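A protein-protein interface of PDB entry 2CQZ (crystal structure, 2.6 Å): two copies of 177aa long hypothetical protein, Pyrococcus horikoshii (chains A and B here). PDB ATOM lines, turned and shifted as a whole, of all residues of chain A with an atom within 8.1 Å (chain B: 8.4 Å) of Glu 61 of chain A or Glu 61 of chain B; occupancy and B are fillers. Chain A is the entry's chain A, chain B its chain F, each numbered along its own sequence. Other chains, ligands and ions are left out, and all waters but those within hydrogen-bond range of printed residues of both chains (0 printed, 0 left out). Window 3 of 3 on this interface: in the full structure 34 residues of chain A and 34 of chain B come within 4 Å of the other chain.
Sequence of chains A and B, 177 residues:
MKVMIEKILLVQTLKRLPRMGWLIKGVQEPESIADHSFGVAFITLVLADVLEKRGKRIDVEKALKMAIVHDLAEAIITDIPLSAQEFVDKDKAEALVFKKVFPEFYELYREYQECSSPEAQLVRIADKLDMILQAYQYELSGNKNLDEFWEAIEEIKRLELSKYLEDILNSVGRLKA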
ATOM      1  N   THR A  44      -4.469  34.186 -22.897  1.00  0.00           N
ATOM      2  CA  THR A  44      -5.254  33.982 -21.685  1.00  0.00           C
ATOM      3  C   THR A  44      -5.443  32.481 -21.460  1.00  0.00           C
ATOM      4  O   THR A  44      -5.287  31.986 -20.345  1.00  0.00           O
ATOM      5  CB  THR A  44      -6.639  34.651 -21.799  1.00  0.00           C
ATOM      6  OG1 THR A  44      -6.478  36.072 -21.852  1.00  0.00           O
ATOM      7  CG2 THR A  44      -7.510  34.289 -20.606  1.00  0.00           C
ATOM      8  N   LEU A  45      -5.773  31.756 -22.524  1.00  0.00           N
ATOM      9  CA  LEU A  45      -5.979  30.317 -22.421  1.00  0.00           C
ATOM     10  C   LEU A  45      -4.703  29.620 -21.964  1.00  0.00           C
ATOM     11  O   LEU A  45      -4.689  28.881 -20.977  1.00  0.00           O
ATOM     12  CB  LEU A  45      -6.427  29.749 -23.776  1.00  0.00           C
ATOM     13  CG  LEU A  45      -6.602  28.229 -23.865  1.00  0.00           C
ATOM     14  CD1 LEU A  45      -7.502  27.727 -22.739  1.00  0.00           C
ATOM     15  CD2 LEU A  45      -7.184  27.873 -25.216  1.00  0.00           C
ATOM     16  N   ALA A  48      -3.707  30.545 -18.399  1.00  0.00           N
ATOM     17  CA  ALA A  48      -4.648  29.960 -17.454  1.00  0.00           C
ATOM     18  C   ALA A  48      -4.235  28.536 -17.095  1.00  0.00           C
ATOM     19  O   ALA A  48      -4.304  28.151 -15.933  1.00  0.00           O
ATOM     20  CB  ALA A  48      -6.048  29.970 -18.038  1.00  0.00           C
ATOM     21  N   ASP A  49      -3.810  27.759 -18.088  1.00  0.00           N
ATOM     22  CA  ASP A  49      -3.369  26.387 -17.854  1.00  0.00           C
ATOM     23  C   ASP A  49      -2.092  26.375 -17.008  1.00  0.00           C
ATOM     24  O   ASP A  49      -1.956  25.559 -16.097  1.00  0.00           O
ATOM     25  CB  ASP A  49      -3.121  25.667 -19.186  1.00  0.00           C
ATOM     26  CG  ASP A  49      -4.410  25.421 -19.970  1.00  0.00           C
ATOM     27  OD1 ASP A  49      -4.336  25.005 -21.155  1.00  0.00           O
ATOM     28  OD2 ASP A  49      -5.504  25.636 -19.399  1.00  0.00           O
ATOM     29  N   GLU A  52      -3.034  27.015 -13.611  1.00  0.00           N
ATOM     30  CA  GLU A  52      -3.698  25.846 -13.027  1.00  0.00           C
ATOM     31  C   GLU A  52      -2.667  24.853 -12.490  1.00  0.00           C
ATOM     32  O   GLU A  52      -2.800  24.371 -11.368  1.00  0.00           O
ATOM     33  CB  GLU A  52      -4.578  25.104 -14.046  1.00  0.00           C
ATOM     34  CG  GLU A  52      -5.732  25.908 -14.656  1.00  0.00           C
ATOM     35  CD  GLU A  52      -6.672  25.027 -15.488  1.00  0.00           C
ATOM     36  OE1 GLU A  52      -6.220  23.959 -15.983  1.00  0.00           O
ATOM     37  OE2 GLU A  52      -7.858  25.400 -15.662  1.00  0.00           O
ATOM     38  N   ARG A  57      -5.702  28.810  -8.820  1.00  0.00           N
ATOM     39  CA  ARG A  57      -6.962  28.465  -9.481  1.00  0.00           C
ATOM     40  C   ARG A  57      -7.587  29.688 -10.145  1.00  0.00           C
ATOM     41  O   ARG A  57      -7.660  30.754  -9.543  1.00  0.00           O
ATOM     42  CB  ARG A  57      -7.971  27.882  -8.488  1.00  0.00           C
ATOM     43  CG  ARG A  57      -9.080  27.014  -9.127  1.00  0.00           C
ATOM     44  CD  ARG A  57      -9.322  27.298 -10.606  1.00  0.00           C
ATOM     45  NE  ARG A  57     -10.580  26.735 -11.079  1.00  0.00           N
ATOM     46  CZ  ARG A  57     -11.773  27.169 -10.681  1.00  0.00           C
ATOM     47  NH1 ARG A  57     -11.866  28.160  -9.793  1.00  0.00           N
ATOM     48  NH2 ARG A  57     -12.879  26.660 -11.219  1.00  0.00           N
ATOM     49  N   ILE A  58      -8.023  29.529 -11.392  1.00  0.00           N
ATOM     50  CA  ILE A  58      -8.649  30.620 -12.142  1.00  0.00           C
ATOM     51  C   ILE A  58     -10.043  30.221 -12.641  1.00  0.00           C
ATOM     52  O   ILE A  58     -10.308  29.043 -12.890  1.00  0.00           O
ATOM     53  CB  ILE A  58      -7.797  31.008 -13.388  1.00  0.00           C
ATOM     54  CG1 ILE A  58      -6.444  31.590 -12.938  1.00  0.00           C
ATOM     55  CG2 ILE A  58      -8.642  31.878 -14.353  1.00  0.00           C
ATOM     56  CD1 ILE A  58      -6.312  33.122 -12.922  1.00  0.00           C
ATOM     57  N   ASP A  59     -10.934  31.206 -12.753  1.00  0.00           N
ATOM     58  CA  ASP A  59     -12.270  30.981 -13.302  1.00  0.00           C
ATOM     59  C   ASP A  59     -12.005  31.167 -14.805  1.00  0.00           C
ATOM     60  O   ASP A  59     -12.152  32.267 -15.353  1.00  0.00           O
ATOM     61  CB  ASP A  59     -13.268  32.044 -12.820  1.00  0.00           C
ATOM     62  CG  ASP A  59     -14.687  31.773 -13.306  1.00  0.00           C
ATOM     63  OD1 ASP A  59     -14.850  31.074 -14.332  1.00  0.00           O
ATOM     64  OD2 ASP A  59     -15.647  32.258 -12.675  1.00  0.00           O
ATOM     65  N   VAL A  60     -11.585  30.089 -15.455  1.00  0.00           N
ATOM     66  CA  VAL A  60     -11.261  30.134 -16.872  1.00  0.00           C
ATOM     67  C   VAL A  60     -12.387  30.658 -17.742  1.00  0.00           C
ATOM     68  O   VAL A  60     -12.148  31.468 -18.639  1.00  0.00           O
ATOM     69  CB  VAL A  60     -10.840  28.754 -17.388  1.00  0.00           C
ATOM     70  CG1 VAL A  60     -10.502  28.838 -18.877  1.00  0.00           C
ATOM     71  CG2 VAL A  60      -9.638  28.261 -16.595  1.00  0.00           C
ATOM     72  N   GLU A  61     -13.610  30.210 -17.488  1.00  0.00           N
ATOM     73  CA  GLU A  61     -14.727  30.678 -18.292  1.00  0.00           C
ATOM     74  C   GLU A  61     -14.787  32.193 -18.254  1.00  0.00           C
ATOM     75  O   GLU A  61     -14.850  32.842 -19.301  1.00  0.00           O
ATOM     76  CB  GLU A  61     -16.053  30.111 -17.795  1.00  0.00           C
ATOM     77  CG  GLU A  61     -17.207  30.383 -18.758  1.00  0.00           C
ATOM     78  CD  GLU A  61     -18.525  29.836 -18.260  1.00  0.00           C
ATOM     79  OE1 GLU A  61     -18.583  28.633 -17.908  1.00  0.00           O
ATOM     80  OE2 GLU A  61     -19.502  30.615 -18.231  1.00  0.00           O
ATOM     81  N   LYS A  62     -14.756  32.763 -17.051  1.00  0.00           N
ATOM     82  CA  LYS A  62     -14.810  34.214 -16.927  1.00  0.00           C
ATOM     83  C   LYS A  62     -13.641  34.894 -17.615  1.00  0.00           C
ATOM     84  O   LYS A  62     -13.811  35.915 -18.281  1.00  0.00           O
ATOM     85  CB  LYS A  62     -14.829  34.658 -15.471  1.00  0.00           C
ATOM     86  CG  LYS A  62     -15.173  36.132 -15.363  1.00  0.00           C
ATOM     87  CD  LYS A  62     -14.699  36.741 -14.074  1.00  0.00           C
ATOM     88  CE  LYS A  62     -15.428  36.195 -12.862  1.00  0.00           C
ATOM     89  NZ  LYS A  62     -14.848  36.835 -11.642  1.00  0.00           N
ATOM     90  N   ALA A  63     -12.447  34.338 -17.455  1.00  0.00           N
ATOM     91  CA  ALA A  63     -11.265  34.922 -18.082  1.00  0.00           C
ATOM     92  C   ALA A  63     -11.390  34.957 -19.607  1.00  0.00           C
ATOM     93  O   ALA A  63     -11.100  35.983 -20.238  1.00  0.00           O
ATOM     94  CB  ALA A  63     -10.020  34.144 -17.685  1.00  0.00           C
ATOM     95  N   LEU A  64     -11.814  33.841 -20.199  1.00  0.00           N
ATOM     96  CA  LEU A  64     -11.951  33.776 -21.647  1.00  0.00           C
ATOM     97  C   LEU A  64     -13.004  34.743 -22.166  1.00  0.00           C
ATOM     98  O   LEU A  64     -12.807  35.370 -23.203  1.00  0.00           O
ATOM     99  CB  LEU A  64     -12.256  32.343 -22.094  1.00  0.00           C
ATOM    100  CG  LEU A  64     -11.099  31.348 -21.921  1.00  0.00           C
ATOM    101  CD1 LEU A  64     -11.524  29.986 -22.437  1.00  0.00           C
ATOM    102  CD2 LEU A  64      -9.855  31.833 -22.675  1.00  0.00           C
ATOM    103  N   LYS A  65     -14.118  34.883 -21.454  1.00  0.00           N
ATOM    104  CA  LYS A  65     -15.148  35.824 -21.889  1.00  0.00           C
ATOM    105  C   LYS A  65     -14.598  37.230 -21.753  1.00  0.00           C
ATOM    106  O   LYS A  65     -14.783  38.071 -22.629  1.00  0.00           O
ATOM    107  CB  LYS A  65     -16.416  35.704 -21.043  1.00  0.00           C
ATOM    108  CG  LYS A  65     -17.229  34.445 -21.273  1.00  0.00           C
ATOM    109  CD  LYS A  65     -18.467  34.471 -20.392  1.00  0.00           C
ATOM    110  CE  LYS A  65     -19.266  33.189 -20.512  1.00  0.00           C
ATOM    111  NZ  LYS A  65     -20.546  33.277 -19.756  1.00  0.00           N
ATOM    112  N   MET A  66     -13.911  37.476 -20.645  1.00  0.00           N
ATOM    113  CA  MET A  66     -13.333  38.788 -20.373  1.00  0.00           C
ATOM    114  C   MET A  66     -12.294  39.161 -21.431  1.00  0.00           C
ATOM    115  O   MET A  66     -12.165  40.323 -21.810  1.00  0.00           O
ATOM    116  CB  MET A  66     -12.706  38.785 -18.981  1.00  0.00           C
ATOM    117  CG  MET A  66     -12.378  40.148 -18.420  1.00  0.00           C
ATOM    118  SD  MET A  66     -11.720  39.997 -16.735  1.00  0.00           S
ATOM    119  CE  MET A  66     -13.255  39.732 -15.778  1.00  0.00           C
ATOM    120  N   ALA A  67     -11.551  38.173 -21.915  1.00  0.00           N
ATOM    121  CA  ALA A  67     -10.551  38.443 -22.941  1.00  0.00           C
ATOM    122  C   ALA A  67     -11.242  38.769 -24.272  1.00  0.00           C
ATOM    123  O   ALA A  67     -10.819  39.662 -24.999  1.00  0.00           O
ATOM    124  CB  ALA A  67      -9.615  37.233 -23.106  1.00  0.00           C
ATOM    125  N   ILE A  68     -12.308  38.041 -24.577  1.00  0.00           N
ATOM    126  CA  ILE A  68     -13.044  38.234 -25.819  1.00  0.00           C
ATOM    127  C   ILE A  68     -13.752  39.588 -25.878  1.00  0.00           C
ATOM    128  O   ILE A  68     -13.810  40.239 -26.927  1.00  0.00           O
ATOM    129  CB  ILE A  68     -14.103  37.115 -26.004  1.00  0.00           C
ATOM    130  CG1 ILE A  68     -13.407  35.777 -26.238  1.00  0.00           C
ATOM    131  CG2 ILE A  68     -15.023  37.449 -27.160  1.00  0.00           C
ATOM    132  CD1 ILE A  68     -14.347  34.587 -26.287  1.00  0.00           C
ATOM    133  N   LEU A 108     -18.379  42.228 -17.024  1.00  0.00           N
ATOM    134  CA  LEU A 108     -17.063  41.732 -17.413  1.00  0.00           C
ATOM    135  C   LEU A 108     -16.148  42.930 -17.651  1.00  0.00           C
ATOM    136  O   LEU A 108     -14.993  42.945 -17.232  1.00  0.00           O
ATOM    137  CB  LEU A 108     -17.162  40.886 -18.683  1.00  0.00           C
ATOM    138  CG  LEU A 108     -17.822  39.518 -18.515  1.00  0.00           C
ATOM    139  CD1 LEU A 108     -18.129  38.894 -19.864  1.00  0.00           C
ATOM    140  CD2 LEU A 108     -16.894  38.627 -17.726  1.00  0.00           C
ATOM    141  N   GLU A 119      -8.702  36.748 -12.588  1.00  0.00           N
ATOM    142  CA  GLU A 119      -9.086  36.735 -13.986  1.00  0.00           C
ATOM    143  C   GLU A 119      -8.785  38.070 -14.648  1.00  0.00           C
ATOM    144  O   GLU A 119      -8.198  38.110 -15.738  1.00  0.00           O
ATOM    145  CB  GLU A 119     -10.576  36.419 -14.136  1.00  0.00           C
ATOM    146  CG  GLU A 119     -11.000  35.056 -13.602  1.00  0.00           C
ATOM    147  CD  GLU A 119     -10.848  34.952 -12.097  1.00  0.00           C
ATOM    148  OE1 GLU A 119     -11.101  35.964 -11.404  1.00  0.00           O
ATOM    149  OE2 GLU A 119     -10.490  33.862 -11.608  1.00  0.00           O
ATOM    150  N   THR B  44     -19.667  32.403 -30.654  1.00  0.00           N
ATOM    151  CA  THR B  44     -19.866  31.258 -29.781  1.00  0.00           C
ATOM    152  C   THR B  44     -20.330  31.758 -28.417  1.00  0.00           C
ATOM    153  O   THR B  44     -21.226  31.177 -27.812  1.00  0.00           O
ATOM    154  CB  THR B  44     -18.586  30.430 -29.608  1.00  0.00           C
ATOM    155  OG1 THR B  44     -18.210  29.864 -30.871  1.00  0.00           O
ATOM    156  CG2 THR B  44     -18.816  29.305 -28.619  1.00  0.00           C
ATOM    157  N   LEU B  45     -19.727  32.839 -27.935  1.00  0.00           N
ATOM    158  CA  LEU B  45     -20.127  33.398 -26.650  1.00  0.00           C
ATOM    159  C   LEU B  45     -21.607  33.794 -26.729  1.00  0.00           C
ATOM    160  O   LEU B  45     -22.446  33.254 -26.011  1.00  0.00           O
ATOM    161  CB  LEU B  45     -19.263  34.624 -26.306  1.00  0.00           C
ATOM    162  CG  LEU B  45     -19.658  35.457 -25.075  1.00  0.00           C
ATOM    163  CD1 LEU B  45     -19.876  34.548 -23.872  1.00  0.00           C
ATOM    164  CD2 LEU B  45     -18.574  36.479 -24.785  1.00  0.00           C
ATOM    165  N   ALA B  48     -24.098  31.000 -27.015  1.00  0.00           N
ATOM    166  CA  ALA B  48     -24.120  30.185 -25.806  1.00  0.00           C
ATOM    167  C   ALA B  48     -25.149  30.749 -24.826  1.00  0.00           C
ATOM    168  O   ALA B  48     -25.923  30.002 -24.231  1.00  0.00           O
ATOM    169  CB  ALA B  48     -22.740  30.159 -25.166  1.00  0.00           C
ATOM    170  N   ASP B  49     -25.154  32.070 -24.673  1.00  0.00           N
ATOM    171  CA  ASP B  49     -26.088  32.732 -23.778  1.00  0.00           C
ATOM    172  C   ASP B  49     -27.532  32.486 -24.243  1.00  0.00           C
ATOM    173  O   ASP B  49     -28.420  32.195 -23.435  1.00  0.00           O
ATOM    174  CB  ASP B  49     -25.775  34.235 -23.729  1.00  0.00           C
ATOM    175  CG  ASP B  49     -24.421  34.540 -23.065  1.00  0.00           C
ATOM    176  OD1 ASP B  49     -23.943  35.694 -23.177  1.00  0.00           O
ATOM    177  OD2 ASP B  49     -23.834  33.633 -22.423  1.00  0.00           O
ATOM    178  N   GLU B  52     -28.487  29.124 -23.429  1.00  0.00           N
ATOM    179  CA  GLU B  52     -28.594  29.095 -21.972  1.00  0.00           C
ATOM    180  C   GLU B  52     -30.016  29.441 -21.525  1.00  0.00           C
ATOM    181  O   GLU B  52     -30.649  28.682 -20.788  1.00  0.00           O
ATOM    182  CB  GLU B  52     -27.588  30.090 -21.359  1.00  0.00           C
ATOM    183  CG  GLU B  52     -28.017  30.749 -20.027  1.00  0.00           C
ATOM    184  CD  GLU B  52     -27.582  29.974 -18.789  1.00  0.00           C
ATOM    185  OE1 GLU B  52     -27.680  28.726 -18.798  1.00  0.00           O
ATOM    186  OE2 GLU B  52     -27.155  30.619 -17.802  1.00  0.00           O
ATOM    187  N   ILE B  58     -24.946  24.387 -21.990  1.00  0.00           N
ATOM    188  CA  ILE B  58     -23.694  24.270 -22.727  1.00  0.00           C
ATOM    189  C   ILE B  58     -22.474  24.425 -21.813  1.00  0.00           C
ATOM    190  O   ILE B  58     -22.461  25.270 -20.930  1.00  0.00           O
ATOM    191  CB  ILE B  58     -23.625  25.374 -23.825  1.00  0.00           C
ATOM    192  CG1 ILE B  58     -24.763  25.181 -24.829  1.00  0.00           C
ATOM    193  CG2 ILE B  58     -22.262  25.364 -24.521  1.00  0.00           C
ATOM    194  CD1 ILE B  58     -24.628  23.921 -25.676  1.00  0.00           C
ATOM    195  N   ASP B  59     -21.454  23.603 -22.018  1.00  0.00           N
ATOM    196  CA  ASP B  59     -20.231  23.731 -21.240  1.00  0.00           C
ATOM    197  C   ASP B  59     -19.505  24.889 -21.920  1.00  0.00           C
ATOM    198  O   ASP B  59     -18.638  24.673 -22.769  1.00  0.00           O
ATOM    199  CB  ASP B  59     -19.393  22.453 -21.349  1.00  0.00           C
ATOM    200  CG  ASP B  59     -18.096  22.526 -20.548  1.00  0.00           C
ATOM    201  OD1 ASP B  59     -17.621  23.648 -20.277  1.00  0.00           O
ATOM    202  OD2 ASP B  59     -17.539  21.457 -20.203  1.00  0.00           O
ATOM    203  N   VAL B  60     -19.879  26.112 -21.561  1.00  0.00           N
ATOM    204  CA  VAL B  60     -19.299  27.318 -22.149  1.00  0.00           C
ATOM    205  C   VAL B  60     -17.780  27.399 -22.154  1.00  0.00           C
ATOM    206  O   VAL B  60     -17.188  27.909 -23.106  1.00  0.00           O
ATOM    207  CB  VAL B  60     -19.823  28.584 -21.459  1.00  0.00           C
ATOM    208  CG1 VAL B  60     -19.314  29.820 -22.192  1.00  0.00           C
ATOM    209  CG2 VAL B  60     -21.339  28.563 -21.440  1.00  0.00           C
ATOM    210  N   GLU B  61     -17.149  26.921 -21.089  1.00  0.00           N
ATOM    211  CA  GLU B  61     -15.695  26.946 -21.010  1.00  0.00           C
ATOM    212  C   GLU B  61     -15.104  26.128 -22.164  1.00  0.00           C
ATOM    213  O   GLU B  61     -14.215  26.597 -22.880  1.00  0.00           O
ATOM    214  CB  GLU B  61     -15.219  26.373 -19.667  1.00  0.00           C
ATOM    215  CG  GLU B  61     -13.693  26.421 -19.483  1.00  0.00           C
ATOM    216  CD  GLU B  61     -13.235  25.866 -18.144  1.00  0.00           C
ATOM    217  OE1 GLU B  61     -13.830  26.247 -17.107  1.00  0.00           O
ATOM    218  OE2 GLU B  61     -12.275  25.065 -18.125  1.00  0.00           O
ATOM    219  N   LYS B  62     -15.603  24.908 -22.339  1.00  0.00           N
ATOM    220  CA  LYS B  62     -15.123  24.035 -23.408  1.00  0.00           C
ATOM    221  C   LYS B  62     -15.385  24.645 -24.780  1.00  0.00           C
ATOM    222  O   LYS B  62     -14.527  24.608 -25.666  1.00  0.00           O
ATOM    223  CB  LYS B  62     -15.809  22.668 -23.359  1.00  0.00           C
ATOM    224  CG  LYS B  62     -15.191  21.689 -24.351  1.00  0.00           C
ATOM    225  CD  LYS B  62     -16.055  20.486 -24.633  1.00  0.00           C
ATOM    226  CE  LYS B  62     -16.161  19.552 -23.463  1.00  0.00           C
ATOM    227  NZ  LYS B  62     -17.004  18.365 -23.821  1.00  0.00           N
ATOM    228  N   ALA B  63     -16.586  25.191 -24.943  1.00  0.00           N
ATOM    229  CA  ALA B  63     -17.000  25.804 -26.191  1.00  0.00           C
ATOM    230  C   ALA B  63     -16.063  26.931 -26.592  1.00  0.00           C
ATOM    231  O   ALA B  63     -15.618  26.988 -27.741  1.00  0.00           O
ATOM    232  CB  ALA B  63     -18.425  26.325 -26.060  1.00  0.00           C
ATOM    233  N   LEU B  64     -15.769  27.825 -25.648  1.00  0.00           N
ATOM    234  CA  LEU B  64     -14.884  28.962 -25.912  1.00  0.00           C
ATOM    235  C   LEU B  64     -13.456  28.512 -26.206  1.00  0.00           C
ATOM    236  O   LEU B  64     -12.775  29.089 -27.056  1.00  0.00           O
ATOM    237  CB  LEU B  64     -14.898  29.942 -24.729  1.00  0.00           C
ATOM    238  CG  LEU B  64     -16.228  30.676 -24.518  1.00  0.00           C
ATOM    239  CD1 LEU B  64     -16.100  31.735 -23.429  1.00  0.00           C
ATOM    240  CD2 LEU B  64     -16.642  31.327 -25.833  1.00  0.00           C
ATOM    241  N   LYS B  65     -12.997  27.483 -25.502  1.00  0.00           N
ATOM    242  CA  LYS B  65     -11.658  26.974 -25.737  1.00  0.00           C
ATOM    243  C   LYS B  65     -11.624  26.392 -27.144  1.00  0.00           C
ATOM    244  O   LYS B  65     -10.716  26.677 -27.926  1.00  0.00           O
ATOM    245  CB  LYS B  65     -11.307  25.899 -24.712  1.00  0.00           C
ATOM    246  CG  LYS B  65     -10.856  26.447 -23.363  1.00  0.00           C
ATOM    247  CD  LYS B  65     -10.435  25.312 -22.435  1.00  0.00           C
ATOM    248  CE  LYS B  65      -9.908  25.837 -21.110  1.00  0.00           C
ATOM    249  NZ  LYS B  65      -9.503  24.707 -20.228  1.00  0.00           N
ATOM    250  N   MET B  66     -12.647  25.599 -27.454  1.00  0.00           N
ATOM    251  CA  MET B  66     -12.804  24.942 -28.749  1.00  0.00           C
ATOM    252  C   MET B  66     -12.860  25.920 -29.913  1.00  0.00           C
ATOM    253  O   MET B  66     -12.364  25.627 -30.990  1.00  0.00           O
ATOM    254  CB  MET B  66     -14.072  24.097 -28.741  1.00  0.00           C
ATOM    255  CG  MET B  66     -14.155  23.096 -29.870  1.00  0.00           C
ATOM    256  SD  MET B  66     -15.576  22.019 -29.661  1.00  0.00           S
ATOM    257  CE  MET B  66     -14.912  20.838 -28.474  1.00  0.00           C
ATOM    258  N   ALA B  67     -13.475  27.074 -29.694  1.00  0.00           N
ATOM    259  CA  ALA B  67     -13.569  28.105 -30.722  1.00  0.00           C
ATOM    260  C   ALA B  67     -12.226  28.818 -30.911  1.00  0.00           C
ATOM    261  O   ALA B  67     -11.898  29.269 -32.003  1.00  0.00           O
ATOM    262  CB  ALA B  67     -14.642  29.124 -30.350  1.00  0.00           C
ATOM    263  N   ILE B  68     -11.450  28.920 -29.840  1.00  0.00           N
ATOM    264  CA  ILE B  68     -10.162  29.591 -29.912  1.00  0.00           C
ATOM    265  C   ILE B  68      -9.105  28.788 -30.674  1.00  0.00           C
ATOM    266  O   ILE B  68      -8.322  29.335 -31.445  1.00  0.00           O
ATOM    267  CB  ILE B  68      -9.645  29.916 -28.483  1.00  0.00           C
ATOM    268  CG1 ILE B  68     -10.492  31.046 -27.890  1.00  0.00           C
ATOM    269  CG2 ILE B  68      -8.178  30.297 -28.512  1.00  0.00           C
ATOM    270  CD1 ILE B  68     -10.247  31.312 -26.415  1.00  0.00           C
ATOM    271  N   LEU B 108      -9.564  18.615 -27.874  1.00  0.00           N
ATOM    272  CA  LEU B 108     -10.541  19.672 -28.142  1.00  0.00           C
ATOM    273  C   LEU B 108     -10.736  19.669 -29.663  1.00  0.00           C
ATOM    274  O   LEU B 108     -11.824  19.939 -30.182  1.00  0.00           O
ATOM    275  CB  LEU B 108     -10.013  21.045 -27.693  1.00  0.00           C
ATOM    276  CG  LEU B 108     -10.070  21.473 -26.225  1.00  0.00           C
ATOM    277  CD1 LEU B 108      -9.433  22.860 -26.058  1.00  0.00           C
ATOM    278  CD2 LEU B 108     -11.518  21.501 -25.777  1.00  0.00           C
ATOM    279  N   GLU B 119     -21.304  21.439 -27.670  1.00  0.00           N
ATOM    280  CA  GLU B 119     -20.204  22.393 -27.779  1.00  0.00           C
ATOM    281  C   GLU B 119     -19.557  22.337 -29.164  1.00  0.00           C
ATOM    282  O   GLU B 119     -19.246  23.370 -29.761  1.00  0.00           O
ATOM    283  CB  GLU B 119     -19.128  22.087 -26.732  1.00  0.00           C
ATOM    284  CG  GLU B 119     -19.522  22.308 -25.270  1.00  0.00           C
ATOM    285  CD  GLU B 119     -20.515  21.280 -24.740  1.00  0.00           C
ATOM    286  OE1 GLU B 119     -20.357  20.071 -25.022  1.00  0.00           O
ATOM    287  OE2 GLU B 119     -21.449  21.692 -24.022  1.00  0.00           O
ATOM    288  N   VAL B 123     -19.646  25.479 -31.965  1.00  0.00           N
ATOM    289  CA  VAL B 123     -18.474  26.100 -32.565  1.00  0.00           C
ATOM    290  C   VAL B 123     -18.587  25.986 -34.089  1.00  0.00           C
ATOM    291  O   VAL B 123     -18.282  26.930 -34.822  1.00  0.00           O
ATOM    292  CB  VAL B 123     -17.176  25.424 -32.048  1.00  0.00           C
ATOM    293  CG1 VAL B 123     -15.936  26.013 -32.716  1.00  0.00           C
ATOM    294  CG2 VAL B 123     -17.095  25.601 -30.547  1.00  0.00           C
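Leu 45 of chain A touches Lys 65 of chain B, and with the chains exchanged Lys 65 of chain A touches Leu 45 of chain B.
Val 60 of chain A touches Glu 61 of chain B, and with the chains exchanged Glu 61 of chain A touches Val 60 of chain B.
Val 60 of chain A touches Lys 65 of chain B, and with the chains exchanged Lys 65 of chain A touches Val 60 of chain B.
Leu 64 of chain A touches Ile 68 of chain B, but with the chains exchanged Ile 68 of chain A does not touch Leu 64 of chain B (4.01 Å).
Positions printed for both chains: 44, 45, 48, 49, 52, 58, 59, 60, 61, 62, 63, 64, 65, 66, 67, 68, 108 and 119.
Of the 19 printed residues of chain A, 5 touch a printed residue of chain B.
Printed residues of chain A that touch a printed residue of chain B: Leu 45, Val 60, Glu 61, Leu 64 and Lys 65.
Hydrophobic or aromatic side chains of chain A that line the printed part of chain B: Leu 45, Val 60 and Leu 64.
Of the 19 printed residues of chain B, 6 touch a printed residue of chain A.
Among the printed residues, no Asp or Glu carboxylate lies within 4 Å of a Lys or Arg side-chain nitrogen of the other chain.
Lys 65 of chain B touches Leu 45 of chain A (CE to CD1, 3.5 Å).
Val 60 of chain A touches Glu 61 of chain B (CB to CD, 3.8 Å).
Val 60 of chain A touches Lys 65 of chain B (CG1 to CE, 3.8 Å).
Glu 61 of chain A touches Val 60 of chain B.
Glu 61 of chain A touches Glu 61 of chain B.
Leu 64 of chain A touches Lys 65 of chain B (CD1 to CG, 3.7 Å).
Leu 64 of chain A touches Ile 68 of chain B.
Lys 65 of chain A touches Leu 45 of chain B (CE to CD1, 3.7 Å).
CE of Lys 65 of chain A touches CG1 of Val 60 of chain B (3.8 Å).
Lys 65 of chain A touches Leu 64 of chain B (CG to CD1, 3.6 Å).
The side-chain carboxylate (OD1) of Asp 59 of chain A lies close to the backbone NH (N) of Glu 61 of chain A (3.5 Å).
The side-chain carboxylate (OE2) of Glu 61 of chain A lies within salt-bridge range of the side-chain amino group (NZ) of Lys 65 of chain A, at 3.2 Å.
The side-chain carboxylate of Asp 59 of chain B sits close to the backbone NH of Glu 61 of chain B, at 3.4 Å.
The side-chain carboxylate (OE2) of Glu 61 of chain B lies within salt-bridge range of the side-chain amino group (NZ) of Lys 65 of chain B (3.5 Å).
Of the printed residues of chain B, Leu 45 of chain A touches Lys 65 (3.5 Å).
Ile 58 of chain A touches none of the printed residues of chain B.
Glu 61 of chain A touches two residues of chain B.
Leu 108 of chain A touches none of the printed residues of chain B.
Of chain A, only Val 60 and Glu 61 come within 4 Å of Glu 61 of chain B.
Of the printed residues of chain A, Lys 65 of chain B touches Leu 45, Val 60 and Leu 64.
Of the printed residues of chain A, Ile 68 of chain B touches Leu 64.
The nearest residue of chain B that does not touch Glu 61 of chain A is Leu 64 of chain B (4.5 Å).
The nearest residue of chain A that does not touch Glu 61 of chain B is Leu 64 of chain A (4.4 Å).
The nearest printed residue of chain B that does not touch Leu 45 of chain A is Ile 68 of chain B (4.2 Å).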
